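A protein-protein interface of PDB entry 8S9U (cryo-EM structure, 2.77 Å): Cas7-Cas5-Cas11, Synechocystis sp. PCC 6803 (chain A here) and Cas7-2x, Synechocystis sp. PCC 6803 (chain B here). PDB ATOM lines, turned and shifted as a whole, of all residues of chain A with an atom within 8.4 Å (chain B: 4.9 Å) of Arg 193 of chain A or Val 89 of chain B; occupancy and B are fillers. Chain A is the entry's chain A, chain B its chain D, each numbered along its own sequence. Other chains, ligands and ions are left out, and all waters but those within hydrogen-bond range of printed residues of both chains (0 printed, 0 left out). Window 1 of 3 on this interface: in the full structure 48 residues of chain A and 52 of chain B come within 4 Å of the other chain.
The backbone NH (N) of Val 89 of chain B lies within hydrogen-bond range of the backbone carbonyl oxygen (O) of Arg 193 of chain A, 2.7 Å away. NH1 of Arg 187 of chain A lies within salt-bridge range of OD1 of Asp 90 of chain B. O of Trp 74 of chain B is in hydrogen-bond range of NH2 of Arg 194 of chain A, at 3.5 Å. The guanidinium group (NH1) of Arg 194 of chain A sits at hydrogen-bond distance from the backbone carbonyl oxygen (O) of Val 87 of chain B, at 2.8 Å. OG of Ser 85 of chain B lies within hydrogen-bond range of NH2 of Arg 194 of chain A (3.1 Å). The backbone NH of Gly 195 of chain A lies close to the backbone carbonyl oxygen of Val 89 of chain B. The backbone carbonyl oxygen of Val 391 of chain A lies within hydrogen-bond range of the backbone NH of Ala 84 of chain B (2.8 Å). The side-chain carboxylate (OD1) of Asp 91 of chain B lies within salt-bridge range of the side-chain amino group (NZ) of Lys 125 of chain A (3.6 Å).
The backbone carbonyl oxygen (O) of Gly 195 of chain A is in hydrogen-bond range of the side-chain hydroxyl (OG) of Ser 12 of chain A. The backbone carbonyl oxygen (O) of Val 87 of chain B sits at hydrogen-bond distance from the side-chain hydroxyl (OG) of Ser 85 of chain B (2.9 Å). O of Asp 389 of chain A sits at hydrogen-bond distance from NE2 of Gln 392 of chain A, 2.8 Å away. The backbone NH (N) of Asp 90 of chain B is in hydrogen-bond range of the backbone carbonyl oxygen (O) of Pro 137 of chain B (3.0 Å). The side-chain carboxylate (OD2) of Asp 50 of chain A sits at hydrogen-bond distance from the side-chain amide nitrogen (NE2) of Gln 392 of chain A (3.5 Å). N of Gly 48 of chain B is in hydrogen-bond range of OD1 of Asp 91 of chain B, at 2.5 Å.
Arg 187 of chain A touches Ile 88 of chain B (CZ to CG2, 3.7 Å). O of Arg 192 of chain A touches CG2 of Ile 88 of chain B, at 3.7 Å. CZ of Arg 193 of chain A touches CB of Ala 84 of chain B (3.8 Å). Arg 193 of chain A touches Val 87 of chain B. CA of Ile 88 of chain B touches O of Arg 193 of chain A, 3.3 Å away. CD of Arg 194 of chain A touches CB of Ala 52 of chain B (3.4 Å). Arg 194 of chain A touches Val 89 of chain B. Gly 195 of chain A touches Asp 90 of chain B. CA of Gly 195 of chain A touches N of Asp 91 of chain B, at 3.5 Å. Gln 392 of chain A touches Ala 84 of chain B (CB to CB, 3.4 Å).
Printed residues of chain B within 4 Å of Lys 125 of chain A: Asp 91 (3.6 Å). Printed residues of chain B within 4 Å of Arg 192 of chain A: Ile 88 (3.7 Å). Arg 193 of chain A touches just these residues of chain B: Ala 84, Val 87, Ile 88 and Val 89. Printed residues of chain B within 4 Å of Arg 194 of chain A: Ala 52 (3.4 Å), Trp 74 (3.5 Å), Ser 85 (3.1 Å), Val 87 (2.8 Å) and Val 89 (3.2 Å). Printed residues of chain A within 4 Å of Trp 74 of chain B: Arg 194 (3.5 Å). Printed residues of chain A within 4 Å of Ala 84 of chain B: Arg 193, Val 391 and Gln 392. Val 89 of chain B touches just these residues of chain A: Arg 193, Arg 194 and Gly 195. Leu 138 of chain B touches none of the printed residues of chain A. The nearest residue of chain B that does not touch Arg 193 of chain A is Ser 85 of chain B (4.1 Å). The nearest residue of chain A that does not touch Val 89 of chain B is Arg 192 of chain A (4.9 Å). The nearest printed residue of chain A that does not touch Trp 74 of chain B is Arg 193 of chain A (6.8 Å).
Of the 23 printed residues of chain A, 8 touch a printed residue of chain B. Among the printed residues, Asp or Glu carboxylates within 4 Å of a Lys or Arg side-chain nitrogen of the other chain: Lys 125 of chain A with Asp 91 of chain B (3.6 Å) and Arg 187 of chain A with Asp 90 of chain B (2.7 Å).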
ATOM      1  N   SER A  12     -17.270  -9.405   5.779  1.00  0.00           N
ATOM      2  CA  SER A  12     -16.889 -10.521   4.946  1.00  0.00           C
ATOM      3  C   SER A  12     -16.194 -11.530   5.831  1.00  0.00           C
ATOM      4  O   SER A  12     -15.842 -11.247   6.973  1.00  0.00           O
ATOM      5  CB  SER A  12     -15.980 -10.102   3.794  1.00  0.00           C
ATOM      6  OG  SER A  12     -14.692  -9.781   4.263  1.00  0.00           O
ATOM      7  N   ILE A  47      -4.479  -2.110  13.776  1.00  0.00           N
ATOM      8  CA  ILE A  47      -5.355  -1.718  12.679  1.00  0.00           C
ATOM      9  C   ILE A  47      -5.906  -0.317  12.885  1.00  0.00           C
ATOM     10  O   ILE A  47      -5.870   0.518  11.979  1.00  0.00           O
ATOM     11  CB  ILE A  47      -6.482  -2.750  12.517  1.00  0.00           C
ATOM     12  CG1 ILE A  47      -5.926  -4.035  11.925  1.00  0.00           C
ATOM     13  CG2 ILE A  47      -7.584  -2.200  11.681  1.00  0.00           C
ATOM     14  CD1 ILE A  47      -5.410  -3.850  10.559  1.00  0.00           C
ATOM     15  N   ASP A  50      -3.151   2.350  12.457  1.00  0.00           N
ATOM     16  CA  ASP A  50      -2.882   2.552  11.038  1.00  0.00           C
ATOM     17  C   ASP A  50      -3.892   3.468  10.367  1.00  0.00           C
ATOM     18  O   ASP A  50      -3.525   4.318   9.554  1.00  0.00           O
ATOM     19  CB  ASP A  50      -2.859   1.203  10.334  1.00  0.00           C
ATOM     20  CG  ASP A  50      -2.377   1.298   8.911  1.00  0.00           C
ATOM     21  OD1 ASP A  50      -3.194   1.615   8.026  1.00  0.00           O
ATOM     22  OD2 ASP A  50      -1.176   1.064   8.670  1.00  0.00           O
ATOM     23  N   LYS A 125     -11.391 -22.137   3.133  1.00  0.00           N
ATOM     24  CA  LYS A 125     -11.310 -21.476   1.840  1.00  0.00           C
ATOM     25  C   LYS A 125     -10.193 -22.101   1.016  1.00  0.00           C
ATOM     26  O   LYS A 125      -9.067 -22.215   1.505  1.00  0.00           O
ATOM     27  CB  LYS A 125     -11.059 -19.992   2.018  1.00  0.00           C
ATOM     28  CG  LYS A 125     -11.209 -19.193   0.764  1.00  0.00           C
ATOM     29  CD  LYS A 125     -11.234 -17.721   1.050  1.00  0.00           C
ATOM     30  CE  LYS A 125     -11.394 -16.938  -0.225  1.00  0.00           C
ATOM     31  NZ  LYS A 125     -11.628 -15.496   0.033  1.00  0.00           N
ATOM     32  N   ARG A 187     -10.883  -2.815   6.800  1.00  0.00           N
ATOM     33  CA  ARG A 187     -10.356  -4.169   6.761  1.00  0.00           C
ATOM     34  C   ARG A 187      -9.435  -4.449   7.931  1.00  0.00           C
ATOM     35  O   ARG A 187      -8.829  -3.540   8.495  1.00  0.00           O
ATOM     36  CB  ARG A 187      -9.535  -4.401   5.502  1.00  0.00           C
ATOM     37  CG  ARG A 187     -10.297  -4.596   4.262  1.00  0.00           C
ATOM     38  CD  ARG A 187      -9.464  -4.145   3.109  1.00  0.00           C
ATOM     39  NE  ARG A 187      -9.953  -2.879   2.595  1.00  0.00           N
ATOM     40  CZ  ARG A 187     -11.104  -2.735   1.952  1.00  0.00           C
ATOM     41  NH1 ARG A 187     -11.900  -3.772   1.769  1.00  0.00           N
ATOM     42  NH2 ARG A 187     -11.473  -1.543   1.517  1.00  0.00           N
ATOM     43  N   LEU A 188      -9.348  -5.725   8.295  1.00  0.00           N
ATOM     44  CA  LEU A 188      -8.467  -6.182   9.352  1.00  0.00           C
ATOM     45  C   LEU A 188      -8.078  -7.625   9.073  1.00  0.00           C
ATOM     46  O   LEU A 188      -8.789  -8.357   8.389  1.00  0.00           O
ATOM     47  CB  LEU A 188      -9.078  -6.015  10.750  1.00  0.00           C
ATOM     48  CG  LEU A 188     -10.327  -6.678  11.301  1.00  0.00           C
ATOM     49  CD1 LEU A 188     -10.081  -8.103  11.696  1.00  0.00           C
ATOM     50  CD2 LEU A 188     -10.752  -5.890  12.484  1.00  0.00           C
ATOM     51  N   GLY A 189      -6.943  -8.022   9.614  1.00  0.00           N
ATOM     52  CA  GLY A 189      -6.504  -9.398   9.570  1.00  0.00           C
ATOM     53  C   GLY A 189      -5.728  -9.768   8.323  1.00  0.00           C
ATOM     54  O   GLY A 189      -5.122  -8.932   7.658  1.00  0.00           O
ATOM     55  N   GLY A 190      -5.752 -11.056   8.005  1.00  0.00           N
ATOM     56  CA  GLY A 190      -4.995 -11.567   6.884  1.00  0.00           C
ATOM     57  C   GLY A 190      -5.784 -11.626   5.591  1.00  0.00           C
ATOM     58  O   GLY A 190      -6.969 -11.934   5.585  1.00  0.00           O
ATOM     59  N   LYS A 191      -5.093 -11.327   4.493  1.00  0.00           N
ATOM     60  CA  LYS A 191      -5.678 -11.275   3.155  1.00  0.00           C
ATOM     61  C   LYS A 191      -6.776 -10.231   3.035  1.00  0.00           C
ATOM     62  O   LYS A 191      -7.778 -10.436   2.357  1.00  0.00           O
ATOM     63  CB  LYS A 191      -6.132 -12.641   2.656  1.00  0.00           C
ATOM     64  CG  LYS A 191      -4.933 -13.511   2.385  1.00  0.00           C
ATOM     65  CD  LYS A 191      -5.080 -14.249   1.074  1.00  0.00           C
ATOM     66  CE  LYS A 191      -3.726 -14.688   0.531  1.00  0.00           C
ATOM     67  NZ  LYS A 191      -2.816 -15.233   1.569  1.00  0.00           N
ATOM     68  N   ARG A 192      -6.590  -9.105   3.716  1.00  0.00           N
ATOM     69  CA  ARG A 192      -7.548  -8.016   3.627  1.00  0.00           C
ATOM     70  C   ARG A 192      -7.668  -7.529   2.204  1.00  0.00           C
ATOM     71  O   ARG A 192      -8.739  -7.088   1.777  1.00  0.00           O
ATOM     72  CB  ARG A 192      -7.063  -6.836   4.423  1.00  0.00           C
ATOM     73  CG  ARG A 192      -6.831  -7.043   5.818  1.00  0.00           C
ATOM     74  CD  ARG A 192      -6.220  -5.778   6.237  1.00  0.00           C
ATOM     75  NE  ARG A 192      -4.945  -6.050   6.834  1.00  0.00           N
ATOM     76  CZ  ARG A 192      -4.181  -5.118   7.344  1.00  0.00           C
ATOM     77  NH1 ARG A 192      -4.576  -3.862   7.302  1.00  0.00           N
ATOM     78  NH2 ARG A 192      -3.022  -5.447   7.868  1.00  0.00           N
ATOM     79  N   ARG A 193      -6.572  -7.587   1.465  1.00  0.00           N
ATOM     80  CA  ARG A 193      -6.516  -7.051   0.123  1.00  0.00           C
ATOM     81  C   ARG A 193      -7.191  -7.979  -0.855  1.00  0.00           C
ATOM     82  O   ARG A 193      -7.551  -7.551  -1.953  1.00  0.00           O
ATOM     83  CB  ARG A 193      -5.063  -6.809  -0.273  1.00  0.00           C
ATOM     84  CG  ARG A 193      -4.513  -5.540   0.303  1.00  0.00           C
ATOM     85  CD  ARG A 193      -3.746  -5.816   1.561  1.00  0.00           C
ATOM     86  NE  ARG A 193      -3.342  -4.583   2.217  1.00  0.00           N
ATOM     87  CZ  ARG A 193      -2.657  -4.539   3.348  1.00  0.00           C
ATOM     88  NH1 ARG A 193      -2.302  -5.655   3.945  1.00  0.00           N
ATOM     89  NH2 ARG A 193      -2.330  -3.382   3.878  1.00  0.00           N
ATOM     90  N   ARG A 194      -7.376  -9.231  -0.471  1.00  0.00           N
ATOM     91  CA  ARG A 194      -8.047 -10.217  -1.289  1.00  0.00           C
ATOM     92  C   ARG A 194      -9.328 -10.641  -0.579  1.00  0.00           C
ATOM     93  O   ARG A 194      -9.476 -11.793  -0.181  1.00  0.00           O
ATOM     94  CB  ARG A 194      -7.149 -11.381  -1.492  1.00  0.00           C
ATOM     95  CG  ARG A 194      -5.833 -11.060  -2.128  1.00  0.00           C
ATOM     96  CD  ARG A 194      -5.981 -10.539  -3.515  1.00  0.00           C
ATOM     97  NE  ARG A 194      -4.713 -10.047  -4.029  1.00  0.00           N
ATOM     98  CZ  ARG A 194      -4.402  -8.772  -4.173  1.00  0.00           C
ATOM     99  NH1 ARG A 194      -5.279  -7.834  -3.882  1.00  0.00           N
ATOM    100  NH2 ARG A 194      -3.221  -8.439  -4.647  1.00  0.00           N
ATOM    101  N   GLY A 195     -10.261  -9.712  -0.443  1.00  0.00           N
ATOM    102  CA  GLY A 195     -11.525  -9.985   0.210  1.00  0.00           C
ATOM    103  C   GLY A 195     -11.689 -10.127   1.710  1.00  0.00           C
ATOM    104  O   GLY A 195     -12.625  -9.547   2.259  1.00  0.00           O
ATOM    105  N   ASN A 196     -10.843 -10.905   2.380  1.00  0.00           N
ATOM    106  CA  ASN A 196     -11.030 -11.185   3.799  1.00  0.00           C
ATOM    107  C   ASN A 196     -11.105  -9.921   4.645  1.00  0.00           C
ATOM    108  O   ASN A 196     -10.638  -8.846   4.267  1.00  0.00           O
ATOM    109  CB  ASN A 196      -9.912 -12.068   4.338  1.00  0.00           C
ATOM    110  CG  ASN A 196     -10.061 -13.498   3.935  1.00  0.00           C
ATOM    111  OD1 ASN A 196     -10.974 -13.855   3.206  1.00  0.00           O
ATOM    112  ND2 ASN A 196      -9.169 -14.337   4.418  1.00  0.00           N
ATOM    113  N   GLY A 197     -11.728 -10.070   5.807  1.00  0.00           N
ATOM    114  CA  GLY A 197     -11.516  -9.174   6.916  1.00  0.00           C
ATOM    115  C   GLY A 197     -12.176  -7.835   6.773  1.00  0.00           C
ATOM    116  O   GLY A 197     -11.803  -6.897   7.468  1.00  0.00           O
ATOM    117  N   ARG A 198     -13.158  -7.723   5.898  1.00  0.00           N
ATOM    118  CA  ARG A 198     -13.916  -6.493   5.774  1.00  0.00           C
ATOM    119  C   ARG A 198     -14.749  -6.282   7.030  1.00  0.00           C
ATOM    120  O   ARG A 198     -15.311  -7.228   7.578  1.00  0.00           O
ATOM    121  CB  ARG A 198     -14.767  -6.576   4.520  1.00  0.00           C
ATOM    122  CG  ARG A 198     -15.371  -5.312   4.055  1.00  0.00           C
ATOM    123  CD  ARG A 198     -16.241  -5.640   2.886  1.00  0.00           C
ATOM    124  NE  ARG A 198     -17.158  -4.566   2.554  1.00  0.00           N
ATOM    125  CZ  ARG A 198     -18.404  -4.768   2.150  1.00  0.00           C
ATOM    126  NH1 ARG A 198     -18.839  -6.000   1.947  1.00  0.00           N
ATOM    127  NH2 ARG A 198     -19.190  -3.738   1.876  1.00  0.00           N
ATOM    128  N   ILE A 387       4.449  -4.355  11.539  1.00  0.00           N
ATOM    129  CA  ILE A 387       4.303  -4.066  10.124  1.00  0.00           C
ATOM    130  C   ILE A 387       5.138  -2.841   9.798  1.00  0.00           C
ATOM    131  O   ILE A 387       5.003  -1.802  10.451  1.00  0.00           O
ATOM    132  CB  ILE A 387       2.826  -3.844   9.780  1.00  0.00           C
ATOM    133  CG1 ILE A 387       2.012  -5.079  10.145  1.00  0.00           C
ATOM    134  CG2 ILE A 387       2.657  -3.447   8.358  1.00  0.00           C
ATOM    135  CD1 ILE A 387       2.312  -6.252   9.365  1.00  0.00           C
ATOM    136  N   GLN A 388       6.001  -2.957   8.798  1.00  0.00           N
ATOM    137  CA  GLN A 388       6.659  -1.793   8.223  1.00  0.00           C
ATOM    138  C   GLN A 388       5.690  -1.064   7.313  1.00  0.00           C
ATOM    139  O   GLN A 388       5.167  -1.652   6.367  1.00  0.00           O
ATOM    140  CB  GLN A 388       7.912  -2.189   7.460  1.00  0.00           C
ATOM    141  CG  GLN A 388       8.695  -0.985   7.029  1.00  0.00           C
ATOM    142  CD  GLN A 388       9.814  -1.321   6.101  1.00  0.00           C
ATOM    143  OE1 GLN A 388      10.716  -2.076   6.449  1.00  0.00           O
ATOM    144  NE2 GLN A 388       9.779  -0.750   4.908  1.00  0.00           N
ATOM    145  N   ASP A 389       5.457   0.215   7.578  1.00  0.00           N
ATOM    146  CA  ASP A 389       4.214   0.829   7.140  1.00  0.00           C
ATOM    147  C   ASP A 389       4.198   1.117   5.650  1.00  0.00           C
ATOM    148  O   ASP A 389       3.121   1.178   5.055  1.00  0.00           O
ATOM    149  CB  ASP A 389       3.980   2.138   7.893  1.00  0.00           C
ATOM    150  CG  ASP A 389       4.356   2.048   9.348  1.00  0.00           C
ATOM    151  OD1 ASP A 389       5.567   2.071   9.639  1.00  0.00           O
ATOM    152  OD2 ASP A 389       3.454   1.964  10.207  1.00  0.00           O
ATOM    153  N   ASP A 390       5.359   1.292   5.025  1.00  0.00           N
ATOM    154  CA  ASP A 390       5.383   1.566   3.594  1.00  0.00           C
ATOM    155  C   ASP A 390       5.225   0.310   2.742  1.00  0.00           C
ATOM    156  O   ASP A 390       4.578   0.357   1.693  1.00  0.00           O
ATOM    157  CB  ASP A 390       6.663   2.309   3.240  1.00  0.00           C
ATOM    158  CG  ASP A 390       7.901   1.535   3.602  1.00  0.00           C
ATOM    159  OD1 ASP A 390       7.787   0.529   4.325  1.00  0.00           O
ATOM    160  OD2 ASP A 390       8.996   1.933   3.162  1.00  0.00           O
ATOM    161  N   VAL A 391       5.819  -0.816   3.143  1.00  0.00           N
ATOM    162  CA  VAL A 391       5.555  -2.081   2.462  1.00  0.00           C
ATOM    163  C   VAL A 391       4.333  -2.797   3.005  1.00  0.00           C
ATOM    164  O   VAL A 391       3.868  -3.759   2.381  1.00  0.00           O
ATOM    165  CB  VAL A 391       6.758  -3.036   2.528  1.00  0.00           C
ATOM    166  CG1 VAL A 391       7.947  -2.407   1.881  1.00  0.00           C
ATOM    167  CG2 VAL A 391       7.066  -3.387   3.936  1.00  0.00           C
ATOM    168  N   GLN A 392       3.805  -2.365   4.140  1.00  0.00           N
ATOM    169  CA  GLN A 392       2.615  -2.936   4.762  1.00  0.00           C
ATOM    170  C   GLN A 392       2.745  -4.424   5.074  1.00  0.00           C
ATOM    171  O   GLN A 392       1.760  -5.151   5.059  1.00  0.00           O
ATOM    172  CB  GLN A 392       1.389  -2.681   3.898  1.00  0.00           C
ATOM    173  CG  GLN A 392       0.894  -1.275   3.953  1.00  0.00           C
ATOM    174  CD  GLN A 392       0.240  -0.952   5.249  1.00  0.00           C
ATOM    175  OE1 GLN A 392      -0.655  -1.655   5.690  1.00  0.00           O
ATOM    176  NE2 GLN A 392       0.685   0.111   5.881  1.00  0.00           N
ATOM    177  N   ARG A 393       3.947  -4.884   5.397  1.00  0.00           N
ATOM    178  CA  ARG A 393       4.204  -6.264   5.783  1.00  0.00           C
ATOM    179  C   ARG A 393       5.369  -6.216   6.746  1.00  0.00           C
ATOM    180  O   ARG A 393       6.156  -5.268   6.695  1.00  0.00           O
ATOM    181  CB  ARG A 393       4.536  -7.192   4.610  1.00  0.00           C
ATOM    182  CG  ARG A 393       5.509  -6.658   3.631  1.00  0.00           C
ATOM    183  CD  ARG A 393       6.069  -7.772   2.821  1.00  0.00           C
ATOM    184  NE  ARG A 393       7.177  -7.318   2.000  1.00  0.00           N
ATOM    185  CZ  ARG A 393       8.447  -7.425   2.347  1.00  0.00           C
ATOM    186  NH1 ARG A 393       8.768  -7.985   3.495  1.00  0.00           N
ATOM    187  NH2 ARG A 393       9.393  -6.984   1.544  1.00  0.00           N
ATOM    188  N   GLY B  48     -12.627 -12.743  -3.529  1.00  0.00           N
ATOM    189  CA  GLY B  48     -11.784 -11.674  -4.018  1.00  0.00           C
ATOM    190  C   GLY B  48     -10.420 -12.160  -4.446  1.00  0.00           C
ATOM    191  O   GLY B  48      -9.778 -11.540  -5.290  1.00  0.00           O
ATOM    192  N   LEU B  51     -11.035 -13.283  -8.109  1.00  0.00           N
ATOM    193  CA  LEU B  51     -11.129 -12.153  -9.025  1.00  0.00           C
ATOM    194  C   LEU B  51      -9.818 -11.387  -9.134  1.00  0.00           C
ATOM    195  O   LEU B  51      -9.476 -10.897 -10.210  1.00  0.00           O
ATOM    196  CB  LEU B  51     -12.249 -11.222  -8.585  1.00  0.00           C
ATOM    197  CG  LEU B  51     -12.491 -10.029  -9.495  1.00  0.00           C
ATOM    198  CD1 LEU B  51     -12.935 -10.482 -10.856  1.00  0.00           C
ATOM    199  CD2 LEU B  51     -13.513  -9.112  -8.882  1.00  0.00           C
ATOM    200  N   ALA B  52      -9.085 -11.249  -8.034  1.00  0.00           N
ATOM    201  CA  ALA B  52      -7.783 -10.599  -8.095  1.00  0.00           C
ATOM    202  C   ALA B  52      -6.840 -11.324  -9.037  1.00  0.00           C
ATOM    203  O   ALA B  52      -6.190 -10.700  -9.881  1.00  0.00           O
ATOM    204  CB  ALA B  52      -7.174 -10.525  -6.704  1.00  0.00           C
ATOM    205  N   TRP B  74       0.097  -4.963  -7.671  1.00  0.00           N
ATOM    206  CA  TRP B  74      -0.485  -6.109  -6.998  1.00  0.00           C
ATOM    207  C   TRP B  74       0.400  -6.603  -5.867  1.00  0.00           C
ATOM    208  O   TRP B  74       0.108  -7.642  -5.276  1.00  0.00           O
ATOM    209  CB  TRP B  74      -0.739  -7.224  -8.014  1.00  0.00           C
ATOM    210  CG  TRP B  74      -1.726  -6.845  -9.088  1.00  0.00           C
ATOM    211  CD1 TRP B  74      -1.430  -6.338 -10.312  1.00  0.00           C
ATOM    212  CD2 TRP B  74      -3.154  -6.936  -9.031  1.00  0.00           C
ATOM    213  NE1 TRP B  74      -2.574  -6.103 -11.019  1.00  0.00           N
ATOM    214  CE2 TRP B  74      -3.648  -6.462 -10.255  1.00  0.00           C
ATOM    215  CE3 TRP B  74      -4.060  -7.371  -8.066  1.00  0.00           C
ATOM    216  CZ2 TRP B  74      -5.001  -6.408 -10.538  1.00  0.00           C
ATOM    217  CZ3 TRP B  74      -5.395  -7.317  -8.350  1.00  0.00           C
ATOM    218  CH2 TRP B  74      -5.857  -6.840  -9.573  1.00  0.00           C
ATOM    219  N   ALA B  84       2.703  -5.198   0.347  1.00  0.00           N
ATOM    220  CA  ALA B  84       1.270  -5.338   0.162  1.00  0.00           C
ATOM    221  C   ALA B  84       0.795  -4.740  -1.153  1.00  0.00           C
ATOM    222  O   ALA B  84       1.434  -3.874  -1.747  1.00  0.00           O
ATOM    223  CB  ALA B  84       0.509  -4.687   1.305  1.00  0.00           C
ATOM    224  N   SER B  85      -0.347  -5.238  -1.607  1.00  0.00           N
ATOM    225  CA  SER B  85      -0.936  -4.834  -2.871  1.00  0.00           C
ATOM    226  C   SER B  85      -1.554  -3.455  -2.768  1.00  0.00           C
ATOM    227  O   SER B  85      -2.034  -3.047  -1.713  1.00  0.00           O
ATOM    228  CB  SER B  85      -2.013  -5.825  -3.278  1.00  0.00           C
ATOM    229  OG  SER B  85      -2.677  -5.402  -4.445  1.00  0.00           O
ATOM    230  N   VAL B  87      -4.047  -2.754  -4.893  1.00  0.00           N
ATOM    231  CA  VAL B  87      -5.399  -3.025  -5.355  1.00  0.00           C
ATOM    232  C   VAL B  87      -6.041  -3.961  -4.350  1.00  0.00           C
ATOM    233  O   VAL B  87      -5.536  -5.062  -4.110  1.00  0.00           O
ATOM    234  CB  VAL B  87      -5.410  -3.639  -6.762  1.00  0.00           C
ATOM    235  CG1 VAL B  87      -6.806  -3.615  -7.328  1.00  0.00           C
ATOM    236  CG2 VAL B  87      -4.498  -2.881  -7.675  1.00  0.00           C
ATOM    237  N   ILE B  88      -7.145  -3.529  -3.758  1.00  0.00           N
ATOM    238  CA  ILE B  88      -7.921  -4.358  -2.850  1.00  0.00           C
ATOM    239  C   ILE B  88      -9.101  -4.915  -3.624  1.00  0.00           C
ATOM    240  O   ILE B  88      -9.829  -4.165  -4.282  1.00  0.00           O
ATOM    241  CB  ILE B  88      -8.404  -3.560  -1.628  1.00  0.00           C
ATOM    242  CG1 ILE B  88      -7.225  -3.009  -0.842  1.00  0.00           C
ATOM    243  CG2 ILE B  88      -9.270  -4.418  -0.748  1.00  0.00           C
ATOM    244  CD1 ILE B  88      -7.459  -1.636  -0.335  1.00  0.00           C
ATOM    245  N   VAL B  89      -9.283  -6.228  -3.559  1.00  0.00           N
ATOM    246  CA  VAL B  89     -10.393  -6.903  -4.211  1.00  0.00           C
ATOM    247  C   VAL B  89     -11.210  -7.580  -3.127  1.00  0.00           C
ATOM    248  O   VAL B  89     -10.713  -8.477  -2.442  1.00  0.00           O
ATOM    249  CB  VAL B  89      -9.908  -7.923  -5.248  1.00  0.00           C
ATOM    250  CG1 VAL B  89     -11.007  -8.222  -6.232  1.00  0.00           C
ATOM    251  CG2 VAL B  89      -8.703  -7.394  -5.968  1.00  0.00           C
ATOM    252  N   ASP B  90     -12.451  -7.148  -2.965  1.00  0.00           N
ATOM    253  CA  ASP B  90     -13.325  -7.737  -1.968  1.00  0.00           C
ATOM    254  C   ASP B  90     -14.046  -8.972  -2.502  1.00  0.00           C
ATOM    255  O   ASP B  90     -14.171  -9.184  -3.706  1.00  0.00           O
ATOM    256  CB  ASP B  90     -14.340  -6.710  -1.475  1.00  0.00           C
ATOM    257  CG  ASP B  90     -13.685  -5.494  -0.871  1.00  0.00           C
ATOM    258  OD1 ASP B  90     -12.867  -5.662   0.053  1.00  0.00           O
ATOM    259  OD2 ASP B  90     -13.979  -4.370  -1.319  1.00  0.00           O
ATOM    260  N   ASP B  91     -14.490  -9.805  -1.570  1.00  0.00           N
ATOM    261  CA  ASP B  91     -15.449 -10.860  -1.858  1.00  0.00           C
ATOM    262  C   ASP B  91     -16.782 -10.264  -2.293  1.00  0.00           C
ATOM    263  O   ASP B  91     -17.294  -9.340  -1.660  1.00  0.00           O
ATOM    264  CB  ASP B  91     -15.637 -11.731  -0.624  1.00  0.00           C
ATOM    265  CG  ASP B  91     -14.415 -12.561  -0.308  1.00  0.00           C
ATOM    266  OD1 ASP B  91     -13.579 -12.760  -1.209  1.00  0.00           O
ATOM    267  OD2 ASP B  91     -14.283 -13.013   0.850  1.00  0.00           O
ATOM    268  N   PRO B 137     -15.788  -5.194  -6.748  1.00  0.00           N
ATOM    269  CA  PRO B 137     -15.311  -4.602  -5.506  1.00  0.00           C
ATOM    270  C   PRO B 137     -13.849  -4.216  -5.530  1.00  0.00           C
ATOM    271  O   PRO B 137     -13.024  -4.941  -4.974  1.00  0.00           O
ATOM    272  CB  PRO B 137     -15.584  -5.721  -4.506  1.00  0.00           C
ATOM    273  CG  PRO B 137     -15.510  -6.996  -5.350  1.00  0.00           C
ATOM    274  CD  PRO B 137     -15.411  -6.607  -6.792  1.00  0.00           C
ATOM    275  N   LEU B 138     -13.494  -3.095  -6.137  1.00  0.00           N
ATOM    276  CA  LEU B 138     -12.093  -2.763  -6.312  1.00  0.00           C
ATOM    277  C   LEU B 138     -11.777  -1.421  -5.686  1.00  0.00           C
ATOM    278  O   LEU B 138     -12.546  -0.465  -5.796  1.00  0.00           O
ATOM    279  CB  LEU B 138     -11.691  -2.709  -7.783  1.00  0.00           C
ATOM    280  CG  LEU B 138     -11.611  -3.966  -8.629  1.00  0.00           C
ATOM    281  CD1 LEU B 138     -11.334  -3.557 -10.048  1.00  0.00           C
ATOM    282  CD2 LEU B 138     -10.519  -4.853  -8.118  1.00  0.00           C
